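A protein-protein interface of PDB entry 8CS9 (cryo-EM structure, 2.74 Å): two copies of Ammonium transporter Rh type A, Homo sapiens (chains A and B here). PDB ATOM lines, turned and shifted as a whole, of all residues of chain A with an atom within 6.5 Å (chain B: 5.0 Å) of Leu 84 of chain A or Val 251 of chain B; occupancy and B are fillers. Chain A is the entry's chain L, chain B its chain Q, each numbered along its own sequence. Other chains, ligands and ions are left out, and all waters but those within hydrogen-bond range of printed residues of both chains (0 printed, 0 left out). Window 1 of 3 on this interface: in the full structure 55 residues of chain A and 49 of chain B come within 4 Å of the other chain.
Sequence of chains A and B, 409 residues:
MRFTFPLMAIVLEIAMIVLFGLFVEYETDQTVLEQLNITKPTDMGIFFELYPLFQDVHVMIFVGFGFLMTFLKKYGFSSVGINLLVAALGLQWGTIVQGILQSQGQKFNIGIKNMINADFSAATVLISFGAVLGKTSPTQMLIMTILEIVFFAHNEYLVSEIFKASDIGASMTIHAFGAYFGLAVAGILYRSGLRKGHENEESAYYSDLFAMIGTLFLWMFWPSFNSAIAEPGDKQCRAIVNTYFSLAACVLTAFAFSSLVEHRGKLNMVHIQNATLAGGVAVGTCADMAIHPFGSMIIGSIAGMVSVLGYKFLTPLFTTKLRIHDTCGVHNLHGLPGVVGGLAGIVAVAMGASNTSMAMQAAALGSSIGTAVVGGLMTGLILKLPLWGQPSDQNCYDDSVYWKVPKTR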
ATOM      1  N   GLU A  13      -4.324 -24.141   1.987  1.00  0.00           N
ATOM      2  CA  GLU A  13      -4.011 -23.567   3.293  1.00  0.00           C
ATOM      3  C   GLU A  13      -2.522 -23.265   3.427  1.00  0.00           C
ATOM      4  O   GLU A  13      -2.141 -22.225   3.978  1.00  0.00           O
ATOM      5  CB  GLU A  13      -4.473 -24.501   4.407  1.00  0.00           C
ATOM      6  CG  GLU A  13      -4.396 -23.868   5.781  1.00  0.00           C
ATOM      7  CD  GLU A  13      -5.113 -22.532   5.839  1.00  0.00           C
ATOM      8  OE1 GLU A  13      -6.328 -22.494   5.558  1.00  0.00           O
ATOM      9  OE2 GLU A  13      -4.459 -21.518   6.158  1.00  0.00           O
ATOM     10  N   PHE A  62     -21.615 -15.735   7.916  1.00  0.00           N
ATOM     11  CA  PHE A  62     -21.549 -17.136   8.310  1.00  0.00           C
ATOM     12  C   PHE A  62     -22.882 -17.724   8.754  1.00  0.00           C
ATOM     13  O   PHE A  62     -23.145 -18.895   8.470  1.00  0.00           O
ATOM     14  CB  PHE A  62     -20.483 -17.320   9.391  1.00  0.00           C
ATOM     15  CG  PHE A  62     -19.091 -17.206   8.854  1.00  0.00           C
ATOM     16  CD1 PHE A  62     -18.433 -18.321   8.365  1.00  0.00           C
ATOM     17  CD2 PHE A  62     -18.463 -15.976   8.774  1.00  0.00           C
ATOM     18  CE1 PHE A  62     -17.161 -18.218   7.845  1.00  0.00           C
ATOM     19  CE2 PHE A  62     -17.194 -15.866   8.251  1.00  0.00           C
ATOM     20  CZ  PHE A  62     -16.543 -16.987   7.782  1.00  0.00           C
ATOM     21  N   GLY A  66     -25.396 -18.970   5.342  1.00  0.00           N
ATOM     22  CA  GLY A  66     -25.288 -20.404   5.562  1.00  0.00           C
ATOM     23  C   GLY A  66     -26.622 -21.063   5.851  1.00  0.00           C
ATOM     24  O   GLY A  66     -26.958 -22.095   5.264  1.00  0.00           O
ATOM     25  N   SER A  78     -24.498 -29.896   3.821  1.00  0.00           N
ATOM     26  CA  SER A  78     -23.651 -29.328   2.784  1.00  0.00           C
ATOM     27  C   SER A  78     -23.807 -27.819   2.715  1.00  0.00           C
ATOM     28  O   SER A  78     -22.812 -27.099   2.624  1.00  0.00           O
ATOM     29  CB  SER A  78     -23.973 -29.960   1.434  1.00  0.00           C
ATOM     30  OG  SER A  78     -23.558 -31.311   1.384  1.00  0.00           O
ATOM     31  N   SER A  79     -25.042 -27.322   2.808  1.00  0.00           N
ATOM     32  CA  SER A  79     -25.279 -25.882   2.763  1.00  0.00           C
ATOM     33  C   SER A  79     -24.454 -25.156   3.819  1.00  0.00           C
ATOM     34  O   SER A  79     -23.560 -24.367   3.491  1.00  0.00           O
ATOM     35  CB  SER A  79     -26.769 -25.591   2.948  1.00  0.00           C
ATOM     36  OG  SER A  79     -27.463 -25.708   1.721  1.00  0.00           O
ATOM     37  N   VAL A  80     -24.691 -25.467   5.094  1.00  0.00           N
ATOM     38  CA  VAL A  80     -24.037 -24.711   6.159  1.00  0.00           C
ATOM     39  C   VAL A  80     -22.533 -25.004   6.207  1.00  0.00           C
ATOM     40  O   VAL A  80     -21.719 -24.083   6.364  1.00  0.00           O
ATOM     41  CB  VAL A  80     -24.747 -24.961   7.507  1.00  0.00           C
ATOM     42  CG1 VAL A  80     -24.549 -26.383   8.011  1.00  0.00           C
ATOM     43  CG2 VAL A  80     -24.283 -23.953   8.542  1.00  0.00           C
ATOM     44  N   GLY A  81     -22.129 -26.266   6.027  1.00  0.00           N
ATOM     45  CA  GLY A  81     -20.720 -26.602   6.155  1.00  0.00           C
ATOM     46  C   GLY A  81     -19.878 -26.064   5.015  1.00  0.00           C
ATOM     47  O   GLY A  81     -18.790 -25.525   5.236  1.00  0.00           O
ATOM     48  N   ILE A  82     -20.355 -26.214   3.778  1.00  0.00           N
ATOM     49  CA  ILE A  82     -19.628 -25.677   2.641  1.00  0.00           C
ATOM     50  C   ILE A  82     -19.678 -24.155   2.650  1.00  0.00           C
ATOM     51  O   ILE A  82     -18.731 -23.506   2.204  1.00  0.00           O
ATOM     52  CB  ILE A  82     -20.170 -26.284   1.332  1.00  0.00           C
ATOM     53  CG1 ILE A  82     -20.025 -27.810   1.351  1.00  0.00           C
ATOM     54  CG2 ILE A  82     -19.442 -25.730   0.132  1.00  0.00           C
ATOM     55  CD1 ILE A  82     -18.656 -28.300   1.785  1.00  0.00           C
ATOM     56  N   ASN A  83     -20.744 -23.556   3.194  1.00  0.00           N
ATOM     57  CA  ASN A  83     -20.732 -22.117   3.430  1.00  0.00           C
ATOM     58  C   ASN A  83     -19.574 -21.725   4.339  1.00  0.00           C
ATOM     59  O   ASN A  83     -18.800 -20.813   4.024  1.00  0.00           O
ATOM     60  CB  ASN A  83     -22.067 -21.686   4.039  1.00  0.00           C
ATOM     61  CG  ASN A  83     -22.226 -20.179   4.114  1.00  0.00           C
ATOM     62  OD1 ASN A  83     -22.828 -19.566   3.235  1.00  0.00           O
ATOM     63  ND2 ASN A  83     -21.707 -19.577   5.178  1.00  0.00           N
ATOM     64  N   LEU A  84     -19.422 -22.435   5.460  1.00  0.00           N
ATOM     65  CA  LEU A  84     -18.345 -22.132   6.398  1.00  0.00           C
ATOM     66  C   LEU A  84     -16.973 -22.334   5.759  1.00  0.00           C
ATOM     67  O   LEU A  84     -16.084 -21.487   5.891  1.00  0.00           O
ATOM     68  CB  LEU A  84     -18.490 -22.997   7.650  1.00  0.00           C
ATOM     69  CG  LEU A  84     -17.287 -23.060   8.594  1.00  0.00           C
ATOM     70  CD1 LEU A  84     -17.054 -21.722   9.284  1.00  0.00           C
ATOM     71  CD2 LEU A  84     -17.465 -24.172   9.614  1.00  0.00           C
ATOM     72  N   LEU A  85     -16.790 -23.449   5.050  1.00  0.00           N
ATOM     73  CA  LEU A  85     -15.499 -23.751   4.435  1.00  0.00           C
ATOM     74  C   LEU A  85     -15.150 -22.741   3.346  1.00  0.00           C
ATOM     75  O   LEU A  85     -14.023 -22.222   3.297  1.00  0.00           O
ATOM     76  CB  LEU A  85     -15.521 -25.171   3.868  1.00  0.00           C
ATOM     77  CG  LEU A  85     -14.435 -25.563   2.866  1.00  0.00           C
ATOM     78  CD1 LEU A  85     -13.098 -25.741   3.559  1.00  0.00           C
ATOM     79  CD2 LEU A  85     -14.829 -26.826   2.125  1.00  0.00           C
ATOM     80  N   VAL A  86     -16.112 -22.446   2.469  1.00  0.00           N
ATOM     81  CA  VAL A  86     -15.894 -21.506   1.380  1.00  0.00           C
ATOM     82  C   VAL A  86     -15.575 -20.126   1.926  1.00  0.00           C
ATOM     83  O   VAL A  86     -14.637 -19.472   1.466  1.00  0.00           O
ATOM     84  CB  VAL A  86     -17.119 -21.487   0.446  1.00  0.00           C
ATOM     85  CG1 VAL A  86     -17.265 -20.140  -0.234  1.00  0.00           C
ATOM     86  CG2 VAL A  86     -17.010 -22.589  -0.586  1.00  0.00           C
ATOM     87  N   ALA A  87     -16.323 -19.669   2.936  1.00  0.00           N
ATOM     88  CA  ALA A  87     -16.069 -18.340   3.479  1.00  0.00           C
ATOM     89  C   ALA A  87     -14.760 -18.280   4.262  1.00  0.00           C
ATOM     90  O   ALA A  87     -14.093 -17.239   4.258  1.00  0.00           O
ATOM     91  CB  ALA A  87     -17.242 -17.900   4.351  1.00  0.00           C
ATOM     92  N   ALA A  88     -14.372 -19.371   4.929  1.00  0.00           N
ATOM     93  CA  ALA A  88     -13.108 -19.380   5.656  1.00  0.00           C
ATOM     94  C   ALA A  88     -11.917 -19.317   4.709  1.00  0.00           C
ATOM     95  O   ALA A  88     -10.956 -18.583   4.964  1.00  0.00           O
ATOM     96  CB  ALA A  88     -13.017 -20.618   6.543  1.00  0.00           C
ATOM     97  N   LEU A  89     -11.954 -20.083   3.616  1.00  0.00           N
ATOM     98  CA  LEU A  89     -10.927 -19.926   2.589  1.00  0.00           C
ATOM     99  C   LEU A  89     -11.012 -18.547   1.948  1.00  0.00           C
ATOM    100  O   LEU A  89      -9.986 -17.930   1.618  1.00  0.00           O
ATOM    101  CB  LEU A  89     -11.071 -21.020   1.531  1.00  0.00           C
ATOM    102  CG  LEU A  89     -10.188 -20.893   0.286  1.00  0.00           C
ATOM    103  CD1 LEU A  89      -8.711 -20.902   0.662  1.00  0.00           C
ATOM    104  CD2 LEU A  89     -10.500 -21.993  -0.712  1.00  0.00           C
ATOM    105  N   LEU A 126     -20.184 -16.632  -1.740  1.00  0.00           N
ATOM    106  CA  LEU A 126     -21.358 -17.349  -1.249  1.00  0.00           C
ATOM    107  C   LEU A 126     -22.581 -17.074  -2.117  1.00  0.00           C
ATOM    108  O   LEU A 126     -23.407 -17.969  -2.345  1.00  0.00           O
ATOM    109  CB  LEU A 126     -21.632 -16.974   0.206  1.00  0.00           C
ATOM    110  CG  LEU A 126     -20.582 -17.447   1.211  1.00  0.00           C
ATOM    111  CD1 LEU A 126     -20.906 -16.944   2.605  1.00  0.00           C
ATOM    112  CD2 LEU A 126     -20.450 -18.962   1.188  1.00  0.00           C
ATOM    113  N   MET B 212     -24.829 -26.883  14.536  1.00  0.00           N
ATOM    114  CA  MET B 212     -24.133 -25.972  13.636  1.00  0.00           C
ATOM    115  C   MET B 212     -24.408 -24.516  13.989  1.00  0.00           C
ATOM    116  O   MET B 212     -23.523 -23.671  13.827  1.00  0.00           O
ATOM    117  CB  MET B 212     -24.526 -26.260  12.189  1.00  0.00           C
ATOM    118  CG  MET B 212     -23.508 -27.096  11.436  1.00  0.00           C
ATOM    119  SD  MET B 212     -21.836 -26.913  12.078  1.00  0.00           S
ATOM    120  CE  MET B 212     -21.307 -25.437  11.215  1.00  0.00           C
ATOM    121  N   LEU B 216     -21.256 -22.150  14.758  1.00  0.00           N
ATOM    122  CA  LEU B 216     -21.020 -20.918  14.022  1.00  0.00           C
ATOM    123  C   LEU B 216     -20.948 -19.723  14.954  1.00  0.00           C
ATOM    124  O   LEU B 216     -20.109 -18.839  14.762  1.00  0.00           O
ATOM    125  CB  LEU B 216     -22.102 -20.722  12.965  1.00  0.00           C
ATOM    126  CG  LEU B 216     -21.930 -21.600  11.727  1.00  0.00           C
ATOM    127  CD1 LEU B 216     -22.950 -21.228  10.676  1.00  0.00           C
ATOM    128  CD2 LEU B 216     -20.516 -21.492  11.179  1.00  0.00           C
ATOM    129  N   TRP B 219     -17.612 -19.798  16.655  1.00  0.00           N
ATOM    130  CA  TRP B 219     -16.557 -19.521  15.688  1.00  0.00           C
ATOM    131  C   TRP B 219     -16.489 -18.041  15.343  1.00  0.00           C
ATOM    132  O   TRP B 219     -15.398 -17.473  15.222  1.00  0.00           O
ATOM    133  CB  TRP B 219     -16.797 -20.351  14.430  1.00  0.00           C
ATOM    134  CG  TRP B 219     -15.644 -20.402  13.503  1.00  0.00           C
ATOM    135  CD1 TRP B 219     -14.646 -21.323  13.489  1.00  0.00           C
ATOM    136  CD2 TRP B 219     -15.367 -19.492  12.435  1.00  0.00           C
ATOM    137  NE1 TRP B 219     -13.758 -21.043  12.483  1.00  0.00           N
ATOM    138  CE2 TRP B 219     -14.180 -19.924  11.817  1.00  0.00           C
ATOM    139  CE3 TRP B 219     -16.009 -18.354  11.942  1.00  0.00           C
ATOM    140  CZ2 TRP B 219     -13.620 -19.258  10.733  1.00  0.00           C
ATOM    141  CZ3 TRP B 219     -15.453 -17.695  10.871  1.00  0.00           C
ATOM    142  CH2 TRP B 219     -14.270 -18.148  10.274  1.00  0.00           C
ATOM    143  N   LEU B 247      -8.678 -19.260  13.233  1.00  0.00           N
ATOM    144  CA  LEU B 247      -9.924 -19.976  12.984  1.00  0.00           C
ATOM    145  C   LEU B 247     -10.125 -20.240  11.497  1.00  0.00           C
ATOM    146  O   LEU B 247     -10.603 -21.317  11.109  1.00  0.00           O
ATOM    147  CB  LEU B 247     -11.099 -19.187  13.556  1.00  0.00           C
ATOM    148  CG  LEU B 247     -11.259 -19.259  15.072  1.00  0.00           C
ATOM    149  CD1 LEU B 247     -12.093 -18.097  15.555  1.00  0.00           C
ATOM    150  CD2 LEU B 247     -11.881 -20.582  15.486  1.00  0.00           C
ATOM    151  N   ALA B 248      -9.760 -19.270  10.651  1.00  0.00           N
ATOM    152  CA  ALA B 248      -9.880 -19.470   9.209  1.00  0.00           C
ATOM    153  C   ALA B 248      -9.033 -20.645   8.728  1.00  0.00           C
ATOM    154  O   ALA B 248      -9.499 -21.469   7.932  1.00  0.00           O
ATOM    155  CB  ALA B 248      -9.487 -18.196   8.471  1.00  0.00           C
ATOM    156  N   ALA B 249      -7.785 -20.738   9.194  1.00  0.00           N
ATOM    157  CA  ALA B 249      -6.939 -21.870   8.812  1.00  0.00           C
ATOM    158  C   ALA B 249      -7.440 -23.175   9.424  1.00  0.00           C
ATOM    159  O   ALA B 249      -7.341 -24.252   8.807  1.00  0.00           O
ATOM    160  CB  ALA B 249      -5.495 -21.600   9.231  1.00  0.00           C
ATOM    161  N   CYS B 250      -7.976 -23.092  10.644  1.00  0.00           N
ATOM    162  CA  CYS B 250      -8.448 -24.276  11.345  1.00  0.00           C
ATOM    163  C   CYS B 250      -9.620 -24.915  10.620  1.00  0.00           C
ATOM    164  O   CYS B 250      -9.746 -26.142  10.604  1.00  0.00           O
ATOM    165  CB  CYS B 250      -8.837 -23.905  12.775  1.00  0.00           C
ATOM    166  SG  CYS B 250      -9.334 -25.287  13.798  1.00  0.00           S
ATOM    167  N   VAL B 251     -10.493 -24.101  10.023  1.00  0.00           N
ATOM    168  CA  VAL B 251     -11.622 -24.658   9.277  1.00  0.00           C
ATOM    169  C   VAL B 251     -11.125 -25.496   8.103  1.00  0.00           C
ATOM    170  O   VAL B 251     -11.597 -26.618   7.873  1.00  0.00           O
ATOM    171  CB  VAL B 251     -12.568 -23.538   8.808  1.00  0.00           C
ATOM    172  CG1 VAL B 251     -13.450 -24.031   7.669  1.00  0.00           C
ATOM    173  CG2 VAL B 251     -13.417 -23.061   9.956  1.00  0.00           C
ATOM    174  N   LEU B 252     -10.157 -24.965   7.350  1.00  0.00           N
ATOM    175  CA  LEU B 252      -9.632 -25.680   6.191  1.00  0.00           C
ATOM    176  C   LEU B 252      -8.999 -26.999   6.602  1.00  0.00           C
ATOM    177  O   LEU B 252      -9.275 -28.049   6.006  1.00  0.00           O
ATOM    178  CB  LEU B 252      -8.613 -24.811   5.451  1.00  0.00           C
ATOM    179  CG  LEU B 252      -9.073 -23.901   4.307  1.00  0.00           C
ATOM    180  CD1 LEU B 252      -9.482 -24.720   3.098  1.00  0.00           C
ATOM    181  CD2 LEU B 252     -10.195 -22.967   4.742  1.00  0.00           C
ATOM    182  N   THR B 253      -8.163 -26.972   7.643  1.00  0.00           N
ATOM    183  CA  THR B 253      -7.504 -28.216   8.034  1.00  0.00           C
ATOM    184  C   THR B 253      -8.476 -29.207   8.666  1.00  0.00           C
ATOM    185  O   THR B 253      -8.331 -30.420   8.468  1.00  0.00           O
ATOM    186  CB  THR B 253      -6.335 -27.933   8.970  1.00  0.00           C
ATOM    187  OG1 THR B 253      -6.725 -26.973   9.958  1.00  0.00           O
ATOM    188  CG2 THR B 253      -5.168 -27.405   8.166  1.00  0.00           C
ATOM    189  N   ALA B 254      -9.471 -28.721   9.414  1.00  0.00           N
ATOM    190  CA  ALA B 254     -10.473 -29.614   9.980  1.00  0.00           C
ATOM    191  C   ALA B 254     -11.277 -30.304   8.889  1.00  0.00           C
ATOM    192  O   ALA B 254     -11.509 -31.514   8.959  1.00  0.00           O
ATOM    193  CB  ALA B 254     -11.395 -28.839  10.921  1.00  0.00           C
ATOM    194  N   PHE B 255     -11.693 -29.556   7.862  1.00  0.00           N
ATOM    195  CA  PHE B 255     -12.408 -30.169   6.746  1.00  0.00           C
ATOM    196  C   PHE B 255     -11.533 -31.181   6.017  1.00  0.00           C
ATOM    197  O   PHE B 255     -11.987 -32.287   5.692  1.00  0.00           O
ATOM    198  CB  PHE B 255     -12.887 -29.090   5.773  1.00  0.00           C
ATOM    199  CG  PHE B 255     -14.313 -28.674   5.980  1.00  0.00           C
ATOM    200  CD1 PHE B 255     -14.631 -27.660   6.869  1.00  0.00           C
ATOM    201  CD2 PHE B 255     -15.336 -29.289   5.279  1.00  0.00           C
ATOM    202  CE1 PHE B 255     -15.941 -27.272   7.058  1.00  0.00           C
ATOM    203  CE2 PHE B 255     -16.649 -28.903   5.465  1.00  0.00           C
ATOM    204  CZ  PHE B 255     -16.951 -27.894   6.355  1.00  0.00           C
ATOM    205  N   ALA B 256     -10.267 -30.825   5.769  1.00  0.00           N
ATOM    206  CA  ALA B 256      -9.373 -31.717   5.036  1.00  0.00           C
ATOM    207  C   ALA B 256      -9.148 -33.021   5.791  1.00  0.00           C
ATOM    208  O   ALA B 256      -9.223 -34.110   5.211  1.00  0.00           O
ATOM    209  CB  ALA B 256      -8.043 -31.013   4.769  1.00  0.00           C
ATOM    210  N   ILE B 272     -16.814 -31.208  11.856  1.00  0.00           N
ATOM    211  CA  ILE B 272     -17.122 -29.855  11.403  1.00  0.00           C
ATOM    212  C   ILE B 272     -17.701 -29.018  12.538  1.00  0.00           C
ATOM    213  O   ILE B 272     -17.472 -27.805  12.606  1.00  0.00           O
ATOM    214  CB  ILE B 272     -18.067 -29.912  10.187  1.00  0.00           C
ATOM    215  CG1 ILE B 272     -17.467 -30.797   9.094  1.00  0.00           C
ATOM    216  CG2 ILE B 272     -18.350 -28.517   9.646  1.00  0.00           C
ATOM    217  CD1 ILE B 272     -16.020 -30.492   8.762  1.00  0.00           C
ATOM    218  N   THR B 276     -13.497 -27.320  14.154  1.00  0.00           N
ATOM    219  CA  THR B 276     -13.346 -26.015  13.523  1.00  0.00           C
ATOM    220  C   THR B 276     -13.109 -24.890  14.525  1.00  0.00           C
ATOM    221  O   THR B 276     -12.772 -23.778  14.108  1.00  0.00           O
ATOM    222  CB  THR B 276     -14.579 -25.698  12.672  1.00  0.00           C
ATOM    223  OG1 THR B 276     -15.767 -25.937  13.436  1.00  0.00           O
ATOM    224  CG2 THR B 276     -14.602 -26.565  11.425  1.00  0.00           C
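NE1 of Trp 219 of chain B lies close to O of Leu 247 of chain B (3.5 Å). The indole nitrogen (NE1) of Trp 219 of chain B lies close to the backbone carbonyl oxygen (O) of Thr 276 of chain B. The side-chain hydroxyl (OG1) of Thr 253 of chain B lies within hydrogen-bond range of the backbone carbonyl oxygen (O) of Ala 249 of chain B (3.0 Å).
Among the printed residues, pairs that only touch across the chains: Glu 13 of chain A with Ala 249 of chain B (3.2 Å), Glu 13 of chain A with Leu 252 of chain B (3.3 Å), Phe 62 of chain A with Leu 216 of chain B (3.2 Å), Phe 62 of chain A with Trp 219 of chain B (3.4 Å), Val 80 of chain A with Met 212 of chain B (3.7 Å), Val 80 of chain A with Leu 216 of chain B (3.7 Å), Gly 81 of chain A with Phe 255 of chain B (3.2 Å), Leu 84 of chain A with Leu 216 of chain B (3.95 Å), Leu 84 of chain A with Val 251 of chain B (3.9 Å), Leu 85 of chain A with Val 251 of chain B (3.8 Å), Leu 85 of chain A with Leu 252 of chain B (3.8 Å), Leu 85 of chain A with Phe 255 of chain B (3.8 Å), Ala 88 of chain A with Ala 248 of chain B (3.8 Å), Ala 88 of chain A with Val 251 of chain B (3.6 Å) and Leu 89 of chain A with Leu 252 of chain B (3.6 Å).
Of the printed residues of chain B, Leu 84 of chain A touches Leu 216 and Val 251. Of chain A, only Leu 84, Leu 85 and Ala 88 come within 4 Å of Val 251 of chain B. Of the printed residues of chain B, Ala 88 of chain A touches Ala 248 (3.8 Å) and Val 251 (3.6 Å). Of the printed residues of chain A, Ala 249 of chain B touches Glu 13 (3.2 Å). Of the printed residues of chain B, Leu 89 of chain A touches Leu 252 (3.6 Å). Ile 82 of chain A touches none of the printed residues of chain B. Ala 256 of chain B touches none of the printed residues of chain A. The nearest residue of chain A that does not touch Val 251 of chain B is Leu 89 of chain A (5.9 Å).
Hydrophobic or aromatic side chains of chain A within 4 Å of the printed part of chain B: Phe 62, Val 80, Leu 84, Leu 85, Ala 88 and Leu 89. Along chain A the printed residues that touch a printed residue of chain B span positions 13 to 89. Hydrophobic or aromatic side chains of chain B within 4 Å of the printed part of chain A: Met 212, Leu 216, Trp 219, Ala 248, Ala 249, Val 251, Leu 252 and Phe 255.
No position is printed for both chains.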
